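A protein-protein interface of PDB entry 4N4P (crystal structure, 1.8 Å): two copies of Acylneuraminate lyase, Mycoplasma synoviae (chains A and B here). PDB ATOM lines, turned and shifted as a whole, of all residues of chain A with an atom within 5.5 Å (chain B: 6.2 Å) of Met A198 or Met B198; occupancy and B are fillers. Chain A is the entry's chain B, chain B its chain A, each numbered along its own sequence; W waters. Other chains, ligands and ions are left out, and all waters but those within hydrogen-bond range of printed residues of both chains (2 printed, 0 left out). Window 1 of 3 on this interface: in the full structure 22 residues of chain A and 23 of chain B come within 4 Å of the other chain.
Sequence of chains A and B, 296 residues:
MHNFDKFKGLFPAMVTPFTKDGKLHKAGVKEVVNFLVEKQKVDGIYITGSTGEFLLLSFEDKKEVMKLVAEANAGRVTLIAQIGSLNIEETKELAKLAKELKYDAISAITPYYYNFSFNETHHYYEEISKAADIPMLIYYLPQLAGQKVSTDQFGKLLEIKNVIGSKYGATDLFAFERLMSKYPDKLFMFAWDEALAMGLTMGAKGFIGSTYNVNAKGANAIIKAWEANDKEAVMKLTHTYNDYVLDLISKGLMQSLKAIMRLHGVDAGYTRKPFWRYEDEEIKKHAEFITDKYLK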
ATOM      1  N   LEU A 173      -7.543  25.021  -6.206  1.00  0.00           N
ATOM      2  CA  LEU A 173      -7.626  23.658  -6.739  1.00  0.00           C
ATOM      3  C   LEU A 173      -6.416  23.312  -7.595  1.00  0.00           C
ATOM      4  O   LEU A 173      -6.090  22.135  -7.796  1.00  0.00           O
ATOM      5  CB  LEU A 173      -8.932  23.439  -7.508  1.00  0.00           C
ATOM      6  CG  LEU A 173     -10.131  23.639  -6.563  1.00  0.00           C
ATOM      7  CD1 LEU A 173     -11.436  23.790  -7.323  1.00  0.00           C
ATOM      8  CD2 LEU A 173     -10.248  22.521  -5.553  1.00  0.00           C
ATOM      9  N   PHE A 174      -5.750  24.345  -8.105  1.00  0.00           N
ATOM     10  CA  PHE A 174      -4.523  24.113  -8.862  1.00  0.00           C
ATOM     11  C   PHE A 174      -3.411  23.655  -7.923  1.00  0.00           C
ATOM     12  O   PHE A 174      -2.751  22.649  -8.177  1.00  0.00           O
ATOM     13  CB  PHE A 174      -4.104  25.364  -9.631  1.00  0.00           C
ATOM     14  CG  PHE A 174      -2.886  25.160 -10.476  1.00  0.00           C
ATOM     15  CD1 PHE A 174      -2.886  24.224 -11.507  1.00  0.00           C
ATOM     16  CD2 PHE A 174      -1.717  25.871 -10.220  1.00  0.00           C
ATOM     17  CE1 PHE A 174      -1.758  24.038 -12.330  1.00  0.00           C
ATOM     18  CE2 PHE A 174      -0.564  25.673 -11.025  1.00  0.00           C
ATOM     19  CZ  PHE A 174      -0.599  24.764 -12.085  1.00  0.00           C
ATOM     20  N   PHE A 176      -3.829  22.042  -5.268  1.00  0.00           N
ATOM     21  CA  PHE A 176      -4.204  20.685  -4.866  1.00  0.00           C
ATOM     22  C   PHE A 176      -3.791  19.683  -5.941  1.00  0.00           C
ATOM     23  O   PHE A 176      -3.175  18.657  -5.648  1.00  0.00           O
ATOM     24  CB  PHE A 176      -5.715  20.561  -4.648  1.00  0.00           C
ATOM     25  CG  PHE A 176      -6.149  19.164  -4.308  1.00  0.00           C
ATOM     26  CD1 PHE A 176      -5.768  18.580  -3.087  1.00  0.00           C
ATOM     27  CD2 PHE A 176      -6.917  18.424  -5.209  1.00  0.00           C
ATOM     28  CE1 PHE A 176      -6.122  17.265  -2.759  1.00  0.00           C
ATOM     29  CE2 PHE A 176      -7.298  17.098  -4.884  1.00  0.00           C
ATOM     30  CZ  PHE A 176      -6.908  16.530  -3.658  1.00  0.00           C
ATOM     31  N   GLU A 177      -4.139  19.993  -7.184  1.00  0.00           N
ATOM     32  CA  GLU A 177      -3.706  19.171  -8.319  1.00  0.00           C
ATOM     33  C   GLU A 177      -2.176  19.010  -8.330  1.00  0.00           C
ATOM     34  O   GLU A 177      -1.676  17.894  -8.544  1.00  0.00           O
ATOM     35  CB  GLU A 177      -4.216  19.766  -9.634  1.00  0.00           C
ATOM     36  CG  GLU A 177      -3.801  18.958 -10.877  1.00  0.00           C
ATOM     37  CD  GLU A 177      -2.386  19.277 -11.358  1.00  0.00           C
ATOM     38  OE1 GLU A 177      -1.978  20.466 -11.311  1.00  0.00           O
ATOM     39  OE2 GLU A 177      -1.716  18.337 -11.853  1.00  0.00           O
ATOM     40  N   PHE A 190      -9.235  15.942   1.796  1.00  0.00           N
ATOM     41  CA  PHE A 190      -9.714  17.134   1.097  1.00  0.00           C
ATOM     42  C   PHE A 190     -10.765  17.813   1.949  1.00  0.00           C
ATOM     43  O   PHE A 190     -11.764  17.188   2.323  1.00  0.00           O
ATOM     44  CB  PHE A 190     -10.304  16.747  -0.266  1.00  0.00           C
ATOM     45  CG  PHE A 190     -10.593  17.919  -1.161  1.00  0.00           C
ATOM     46  CD1 PHE A 190      -9.583  18.497  -1.935  1.00  0.00           C
ATOM     47  CD2 PHE A 190     -11.895  18.459  -1.220  1.00  0.00           C
ATOM     48  CE1 PHE A 190      -9.849  19.605  -2.766  1.00  0.00           C
ATOM     49  CE2 PHE A 190     -12.177  19.550  -2.058  1.00  0.00           C
ATOM     50  CZ  PHE A 190     -11.168  20.122  -2.835  1.00  0.00           C
ATOM     51  N   ALA A 195     -16.328  21.809  -2.817  1.00  0.00           N
ATOM     52  CA  ALA A 195     -15.569  21.371  -4.010  1.00  0.00           C
ATOM     53  C   ALA A 195     -15.312  19.863  -3.959  1.00  0.00           C
ATOM     54  O   ALA A 195     -14.379  19.367  -4.598  1.00  0.00           O
ATOM     55  CB  ALA A 195     -14.223  22.135  -4.079  1.00  0.00           C
ATOM     56  N   LEU A 196     -16.143  19.147  -3.195  1.00  0.00           N
ATOM     57  CA  LEU A 196     -16.053  17.679  -3.059  1.00  0.00           C
ATOM     58  C   LEU A 196     -15.784  16.997  -4.408  1.00  0.00           C
ATOM     59  O   LEU A 196     -14.779  16.286  -4.559  1.00  0.00           O
ATOM     60  CB  LEU A 196     -17.321  17.100  -2.365  1.00  0.00           C
ATOM     61  CG  LEU A 196     -17.129  15.715  -1.715  1.00  0.00           C
ATOM     62  CD1 LEU A 196     -18.274  15.434  -0.754  1.00  0.00           C
ATOM     63  CD2 LEU A 196     -17.055  14.621  -2.790  1.00  0.00           C
ATOM     64  N   ALA A 197     -16.673  17.220  -5.376  1.00  0.00           N
ATOM     65  CA  ALA A 197     -16.533  16.600  -6.698  1.00  0.00           C
ATOM     66  C   ALA A 197     -15.242  16.992  -7.438  1.00  0.00           C
ATOM     67  O   ALA A 197     -14.652  16.144  -8.135  1.00  0.00           O
ATOM     68  CB  ALA A 197     -17.770  16.852  -7.560  1.00  0.00           C
ATOM     69  N   MET A 198     -14.776  18.235  -7.248  1.00  0.00           N
ATOM     70  CA  MET A 198     -13.499  18.685  -7.834  1.00  0.00           C
ATOM     71  C   MET A 198     -12.349  17.889  -7.219  1.00  0.00           C
ATOM     72  O   MET A 198     -11.437  17.464  -7.941  1.00  0.00           O
ATOM     73  CB  MET A 198     -13.212  20.182  -7.587  1.00  0.00           C
ATOM     74  CG  MET A 198     -14.344  21.177  -7.917  1.00  0.00           C
ATOM     75  SD  MET A 198     -14.503  21.269  -9.693  1.00  0.00           S
ATOM     76  CE  MET A 198     -15.642  19.941 -10.082  1.00  0.00           C
ATOM     77  N   GLY A 199     -12.395  17.709  -5.895  1.00  0.00           N
ATOM     78  CA  GLY A 199     -11.398  16.910  -5.171  1.00  0.00           C
ATOM     79  C   GLY A 199     -11.343  15.482  -5.713  1.00  0.00           C
ATOM     80  O   GLY A 199     -10.264  14.955  -5.975  1.00  0.00           O
ATOM     81  N   LEU A 200     -12.513  14.859  -5.838  1.00  0.00           N
ATOM     82  CA  LEU A 200     -12.637  13.496  -6.369  1.00  0.00           C
ATOM     83  C   LEU A 200     -11.999  13.391  -7.758  1.00  0.00           C
ATOM     84  O   LEU A 200     -11.245  12.446  -8.043  1.00  0.00           O
ATOM     85  CB  LEU A 200     -14.107  13.122  -6.470  1.00  0.00           C
ATOM     86  CG  LEU A 200     -14.855  12.623  -5.225  1.00  0.00           C
ATOM     87  CD1 LEU A 200     -16.335  12.534  -5.555  1.00  0.00           C
ATOM     88  CD2 LEU A 200     -14.357  11.271  -4.679  1.00  0.00           C
ATOM     89  N   THR A 201     -12.286  14.383  -8.585  1.00  0.00           N
ATOM     90  CA  THR A 201     -11.776  14.427  -9.955  1.00  0.00           C
ATOM     91  C   THR A 201     -10.265  14.341  -9.990  1.00  0.00           C
ATOM     92  O   THR A 201      -9.705  13.652 -10.848  1.00  0.00           O
ATOM     93  CB  THR A 201     -12.221  15.718 -10.679  1.00  0.00           C
ATOM     94  OG1 THR A 201     -13.646  15.736 -10.682  1.00  0.00           O
ATOM     95  CG2 THR A 201     -11.760  15.717 -12.189  1.00  0.00           C
ATOM     96  N   MET A 202      -9.624  15.037  -9.063  1.00  0.00           N
ATOM     97  CA  MET A 202      -8.152  15.034  -9.020  1.00  0.00           C
ATOM     98  C   MET A 202      -7.553  14.017  -8.040  1.00  0.00           C
ATOM     99  O   MET A 202      -6.357  14.096  -7.715  1.00  0.00           O
ATOM    100  CB  MET A 202      -7.569  16.457  -8.845  1.00  0.00           C
ATOM    101  CG  MET A 202      -7.113  17.166 -10.212  1.00  0.00           C
ATOM    102  SD  MET A 202      -6.307  15.996 -11.383  1.00  0.00           S
ATOM    103  CE  MET A 202      -7.653  15.913 -12.591  1.00  0.00           C
ATOM    104  N   GLY A 203      -8.360  13.058  -7.581  1.00  0.00           N
ATOM    105  CA  GLY A 203      -7.820  11.926  -6.855  1.00  0.00           C
ATOM    106  C   GLY A 203      -8.000  11.879  -5.337  1.00  0.00           C
ATOM    107  O   GLY A 203      -7.507  10.958  -4.692  1.00  0.00           O
ATOM    108  N   LEU B 173     -13.535  28.031  -8.873  1.00  0.00           N
ATOM    109  CA  LEU B 173     -14.418  26.979  -9.366  1.00  0.00           C
ATOM    110  C   LEU B 173     -15.744  26.889  -8.613  1.00  0.00           C
ATOM    111  O   LEU B 173     -16.682  26.276  -9.116  1.00  0.00           O
ATOM    112  CB  LEU B 173     -13.721  25.634  -9.419  1.00  0.00           C
ATOM    113  CG  LEU B 173     -12.485  25.657 -10.355  1.00  0.00           C
ATOM    114  CD1 LEU B 173     -11.944  24.286 -10.506  1.00  0.00           C
ATOM    115  CD2 LEU B 173     -12.793  26.217 -11.724  1.00  0.00           C
ATOM    116  N   PHE B 176     -17.968  29.237 -10.498  1.00  0.00           N
ATOM    117  CA  PHE B 176     -18.312  28.565 -11.738  1.00  0.00           C
ATOM    118  C   PHE B 176     -19.466  27.601 -11.489  1.00  0.00           C
ATOM    119  O   PHE B 176     -20.450  27.547 -12.243  1.00  0.00           O
ATOM    120  CB  PHE B 176     -17.127  27.795 -12.339  1.00  0.00           C
ATOM    121  CG  PHE B 176     -17.482  27.096 -13.631  1.00  0.00           C
ATOM    122  CD1 PHE B 176     -17.868  27.837 -14.746  1.00  0.00           C
ATOM    123  CD2 PHE B 176     -17.506  25.704 -13.705  1.00  0.00           C
ATOM    124  CE1 PHE B 176     -18.251  27.206 -15.953  1.00  0.00           C
ATOM    125  CE2 PHE B 176     -17.866  25.054 -14.910  1.00  0.00           C
ATOM    126  CZ  PHE B 176     -18.239  25.811 -16.028  1.00  0.00           C
ATOM    127  N   PHE B 190     -15.352  27.493 -20.860  1.00  0.00           N
ATOM    128  CA  PHE B 190     -14.435  27.410 -19.715  1.00  0.00           C
ATOM    129  C   PHE B 190     -12.999  27.787 -20.154  1.00  0.00           C
ATOM    130  O   PHE B 190     -12.440  27.170 -21.055  1.00  0.00           O
ATOM    131  CB  PHE B 190     -14.498  26.012 -19.108  1.00  0.00           C
ATOM    132  CG  PHE B 190     -13.843  25.909 -17.772  1.00  0.00           C
ATOM    133  CD1 PHE B 190     -14.524  26.303 -16.617  1.00  0.00           C
ATOM    134  CD2 PHE B 190     -12.536  25.447 -17.663  1.00  0.00           C
ATOM    135  CE1 PHE B 190     -13.906  26.229 -15.367  1.00  0.00           C
ATOM    136  CE2 PHE B 190     -11.910  25.342 -16.416  1.00  0.00           C
ATOM    137  CZ  PHE B 190     -12.585  25.736 -15.269  1.00  0.00           C
ATOM    138  N   TRP B 192     -10.037  28.303 -18.174  1.00  0.00           N
ATOM    139  CA  TRP B 192      -8.887  28.087 -17.292  1.00  0.00           C
ATOM    140  C   TRP B 192      -8.273  26.719 -17.604  1.00  0.00           C
ATOM    141  O   TRP B 192      -8.732  25.692 -17.127  1.00  0.00           O
ATOM    142  CB  TRP B 192      -9.261  28.262 -15.811  1.00  0.00           C
ATOM    143  CG  TRP B 192      -8.067  28.075 -14.864  1.00  0.00           C
ATOM    144  CD1 TRP B 192      -6.748  28.278 -15.146  1.00  0.00           C
ATOM    145  CD2 TRP B 192      -8.124  27.650 -13.498  1.00  0.00           C
ATOM    146  NE1 TRP B 192      -5.963  28.003 -14.022  1.00  0.00           N
ATOM    147  CE2 TRP B 192      -6.789  27.632 -12.999  1.00  0.00           C
ATOM    148  CE3 TRP B 192      -9.169  27.303 -12.639  1.00  0.00           C
ATOM    149  CZ2 TRP B 192      -6.487  27.271 -11.688  1.00  0.00           C
ATOM    150  CZ3 TRP B 192      -8.862  26.930 -11.333  1.00  0.00           C
ATOM    151  CH2 TRP B 192      -7.533  26.914 -10.877  1.00  0.00           C
ATOM    152  N   GLU B 194      -5.663  25.032 -16.941  1.00  0.00           N
ATOM    153  CA  GLU B 194      -5.154  24.130 -15.898  1.00  0.00           C
ATOM    154  C   GLU B 194      -6.249  23.405 -15.098  1.00  0.00           C
ATOM    155  O   GLU B 194      -5.964  22.579 -14.232  1.00  0.00           O
ATOM    156  CB  GLU B 194      -4.255  24.911 -14.952  1.00  0.00           C
ATOM    157  CG  GLU B 194      -3.039  25.483 -15.649  1.00  0.00           C
ATOM    158  CD  GLU B 194      -2.406  26.647 -14.879  1.00  0.00           C
ATOM    159  OE1 GLU B 194      -3.129  27.366 -14.134  1.00  0.00           O
ATOM    160  OE2 GLU B 194      -1.170  26.827 -15.016  1.00  0.00           O
ATOM    161  N   ALA B 195      -7.500  23.714 -15.389  1.00  0.00           N
ATOM    162  CA  ALA B 195      -8.588  23.105 -14.633  1.00  0.00           C
ATOM    163  C   ALA B 195      -9.608  22.469 -15.542  1.00  0.00           C
ATOM    164  O   ALA B 195     -10.781  22.326 -15.169  1.00  0.00           O
ATOM    165  CB  ALA B 195      -9.245  24.142 -13.737  1.00  0.00           C
ATOM    166  N   LEU B 196      -9.155  22.081 -16.736  1.00  0.00           N
ATOM    167  CA  LEU B 196     -10.037  21.529 -17.764  1.00  0.00           C
ATOM    168  C   LEU B 196     -10.969  20.446 -17.212  1.00  0.00           C
ATOM    169  O   LEU B 196     -12.210  20.508 -17.392  1.00  0.00           O
ATOM    170  CB  LEU B 196      -9.192  20.978 -18.935  1.00  0.00           C
ATOM    171  CG  LEU B 196      -9.948  20.806 -20.269  1.00  0.00           C
ATOM    172  CD1 LEU B 196      -8.964  20.728 -21.446  1.00  0.00           C
ATOM    173  CD2 LEU B 196     -10.829  19.576 -20.302  1.00  0.00           C
ATOM    174  N   ALA B 197     -10.374  19.446 -16.564  1.00  0.00           N
ATOM    175  CA  ALA B 197     -11.137  18.303 -16.065  1.00  0.00           C
ATOM    176  C   ALA B 197     -12.086  18.713 -14.944  1.00  0.00           C
ATOM    177  O   ALA B 197     -13.178  18.168 -14.813  1.00  0.00           O
ATOM    178  CB  ALA B 197     -10.203  17.201 -15.604  1.00  0.00           C
ATOM    179  N   MET B 198     -11.691  19.695 -14.156  1.00  0.00           N
ATOM    180  CA  MET B 198     -12.577  20.195 -13.125  1.00  0.00           C
ATOM    181  C   MET B 198     -13.773  20.929 -13.770  1.00  0.00           C
ATOM    182  O   MET B 198     -14.915  20.788 -13.317  1.00  0.00           O
ATOM    183  CB  MET B 198     -11.780  21.005 -12.105  1.00  0.00           C
ATOM    184  CG  MET B 198     -10.978  20.067 -11.093  1.00  0.00           C
ATOM    185  SD  MET B 198     -10.022  21.143 -10.110  1.00  0.00           S
ATOM    186  CE  MET B 198      -8.809  20.020  -9.380  1.00  0.00           C
ATOM    187  N   GLY B 199     -13.498  21.689 -14.840  1.00  0.00           N
ATOM    188  CA  GLY B 199     -14.547  22.333 -15.637  1.00  0.00           C
ATOM    189  C   GLY B 199     -15.521  21.295 -16.213  1.00  0.00           C
ATOM    190  O   GLY B 199     -16.750  21.446 -16.091  1.00  0.00           O
ATOM    191  N   LEU B 200     -14.996  20.258 -16.864  1.00  0.00           N
ATOM    192  CA  LEU B 200     -15.855  19.180 -17.389  1.00  0.00           C
ATOM    193  C   LEU B 200     -16.749  18.592 -16.313  1.00  0.00           C
ATOM    194  O   LEU B 200     -17.933  18.355 -16.535  1.00  0.00           O
ATOM    195  CB  LEU B 200     -15.017  18.031 -17.949  1.00  0.00           C
ATOM    196  CG  LEU B 200     -14.319  18.225 -19.299  1.00  0.00           C
ATOM    197  CD1 LEU B 200     -13.282  17.135 -19.369  1.00  0.00           C
ATOM    198  CD2 LEU B 200     -15.297  18.165 -20.487  1.00  0.00           C
ATOM    199  N   THR B 201     -16.152  18.326 -15.157  1.00  0.00           N
ATOM    200  CA  THR B 201     -16.862  17.716 -14.032  1.00  0.00           C
ATOM    201  C   THR B 201     -18.062  18.561 -13.581  1.00  0.00           C
ATOM    202  O   THR B 201     -19.066  18.022 -13.143  1.00  0.00           O
ATOM    203  CB  THR B 201     -15.894  17.416 -12.878  1.00  0.00           C
ATOM    204  OG1 THR B 201     -14.911  16.476 -13.353  1.00  0.00           O
ATOM    205  CG2 THR B 201     -16.652  16.789 -11.680  1.00  0.00           C
ATOM    206  N   MET B 202     -17.966  19.881 -13.717  1.00  0.00           N
ATOM    207  CA  MET B 202     -19.104  20.719 -13.369  1.00  0.00           C
ATOM    208  C   MET B 202     -19.960  21.150 -14.586  1.00  0.00           C
ATOM    209  O   MET B 202     -20.827  22.036 -14.466  1.00  0.00           O
ATOM    210  CB  MET B 202     -18.670  21.896 -12.472  1.00  0.00           C
ATOM    211  CG  MET B 202     -19.793  22.339 -11.486  1.00  0.00           C
ATOM    212  SD  MET B 202     -20.721  20.989 -10.693  1.00  0.00           S
ATOM    213  CE  MET B 202     -19.455  19.894  -9.993  1.00  0.00           C
ATOM    214  N   GLY B 203     -19.735  20.515 -15.741  1.00  0.00           N
ATOM    215  CA  GLY B 203     -20.649  20.693 -16.888  1.00  0.00           C
ATOM    216  C   GLY B 203     -20.171  21.529 -18.066  1.00  0.00           C
ATOM    217  O   GLY B 203     -20.902  21.723 -19.022  1.00  0.00           O
HETATM  218  O   HOH W   1     -16.963  23.598  -9.912  1.00  0.00           O
HETATM  219  O   HOH W   2     -14.967  13.663 -12.638  1.00  0.00           O
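OG1 of Thr A201 is in hydrogen-bond range of OG1 of Thr B201, 3.0 Å away. The side-chain sulfur of Met A198 sits close to the backbone carbonyl oxygen of Met B198, 3.7 Å away.
The backbone carbonyl oxygen (O) of Ala B197 lies within hydrogen-bond range of the side-chain hydroxyl (OG1) of Thr B201 (2.8 Å). The backbone carbonyl oxygen (O) of Ala A197 sits at hydrogen-bond distance from the side-chain hydroxyl (OG1) of Thr A201 (2.8 Å). The indole nitrogen of Trp B192 is in hydrogen-bond range of the side-chain carboxylate of Glu B194, 2.9 Å away.
Among the printed residues, pairs that only touch across the chains: Leu A173 with Leu B173 (3.3 Å), Met A202 with Met B198 (3.4 Å), Phe A174 with Glu B194 (3.6 Å), Leu A173 with Met B198 (3.6 Å), Met A198 with Thr B201 (3.7 Å), Phe A174 with Trp B192 (3.7 Å), Met A198 with Met B202 (3.8 Å) and Thr A201 with Ala B197 (3.9 Å).
Of chain B, only Met B198, Thr B201 and Met B202 come within 4 Å of Met A198. Printed residues of chain A within 4 Å of Met B198: Leu A173 (3.6 Å), Met A198 (3.4 Å) and Met A202 (3.4 Å). Of the printed residues of chain A, Thr B201 touches Met A198 (3.7 Å) and Thr A201 (3.0 Å). Printed residues of chain A within 4 Å of Leu B173: Leu A173. Ala A195 touches none of the printed residues of chain B. The nearest residue of chain B that does not touch Met A198 is Leu B173 (4.04 Å). The nearest residue of chain A that does not touch Met B198 is Thr A201 (4.4 Å).
Among the printed residues, 10 pairs touch across the chains.
Leu B173 touches its own counterpart, Leu A173. Met A198 touches Thr B201, but with the chains exchanged Thr A201 does not touch Met B198 (4.4 Å). Met A198 touches Met B202, and with the chains exchanged Met A202 touches Met B198. Thr A201 touches its own counterpart, Thr B201. Positions printed for both chains: 173, 176, 190, 195, 196, 197, 198, 199, 200, 201, 202 and 203. Of the 10 pairs that touch across the chains among the printed residues, 5 have their exchanged pair printed and touching as well.
Water W1 lies within hydrogen-bond range of O of Leu B173 and SD of Met A198. Water W2 lies within hydrogen-bond range of the side-chain hydroxyl (OG1) of Thr B201 (2.9 Å) and the side-chain hydroxyl (OG1) of Thr A201 (3.1 Å).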
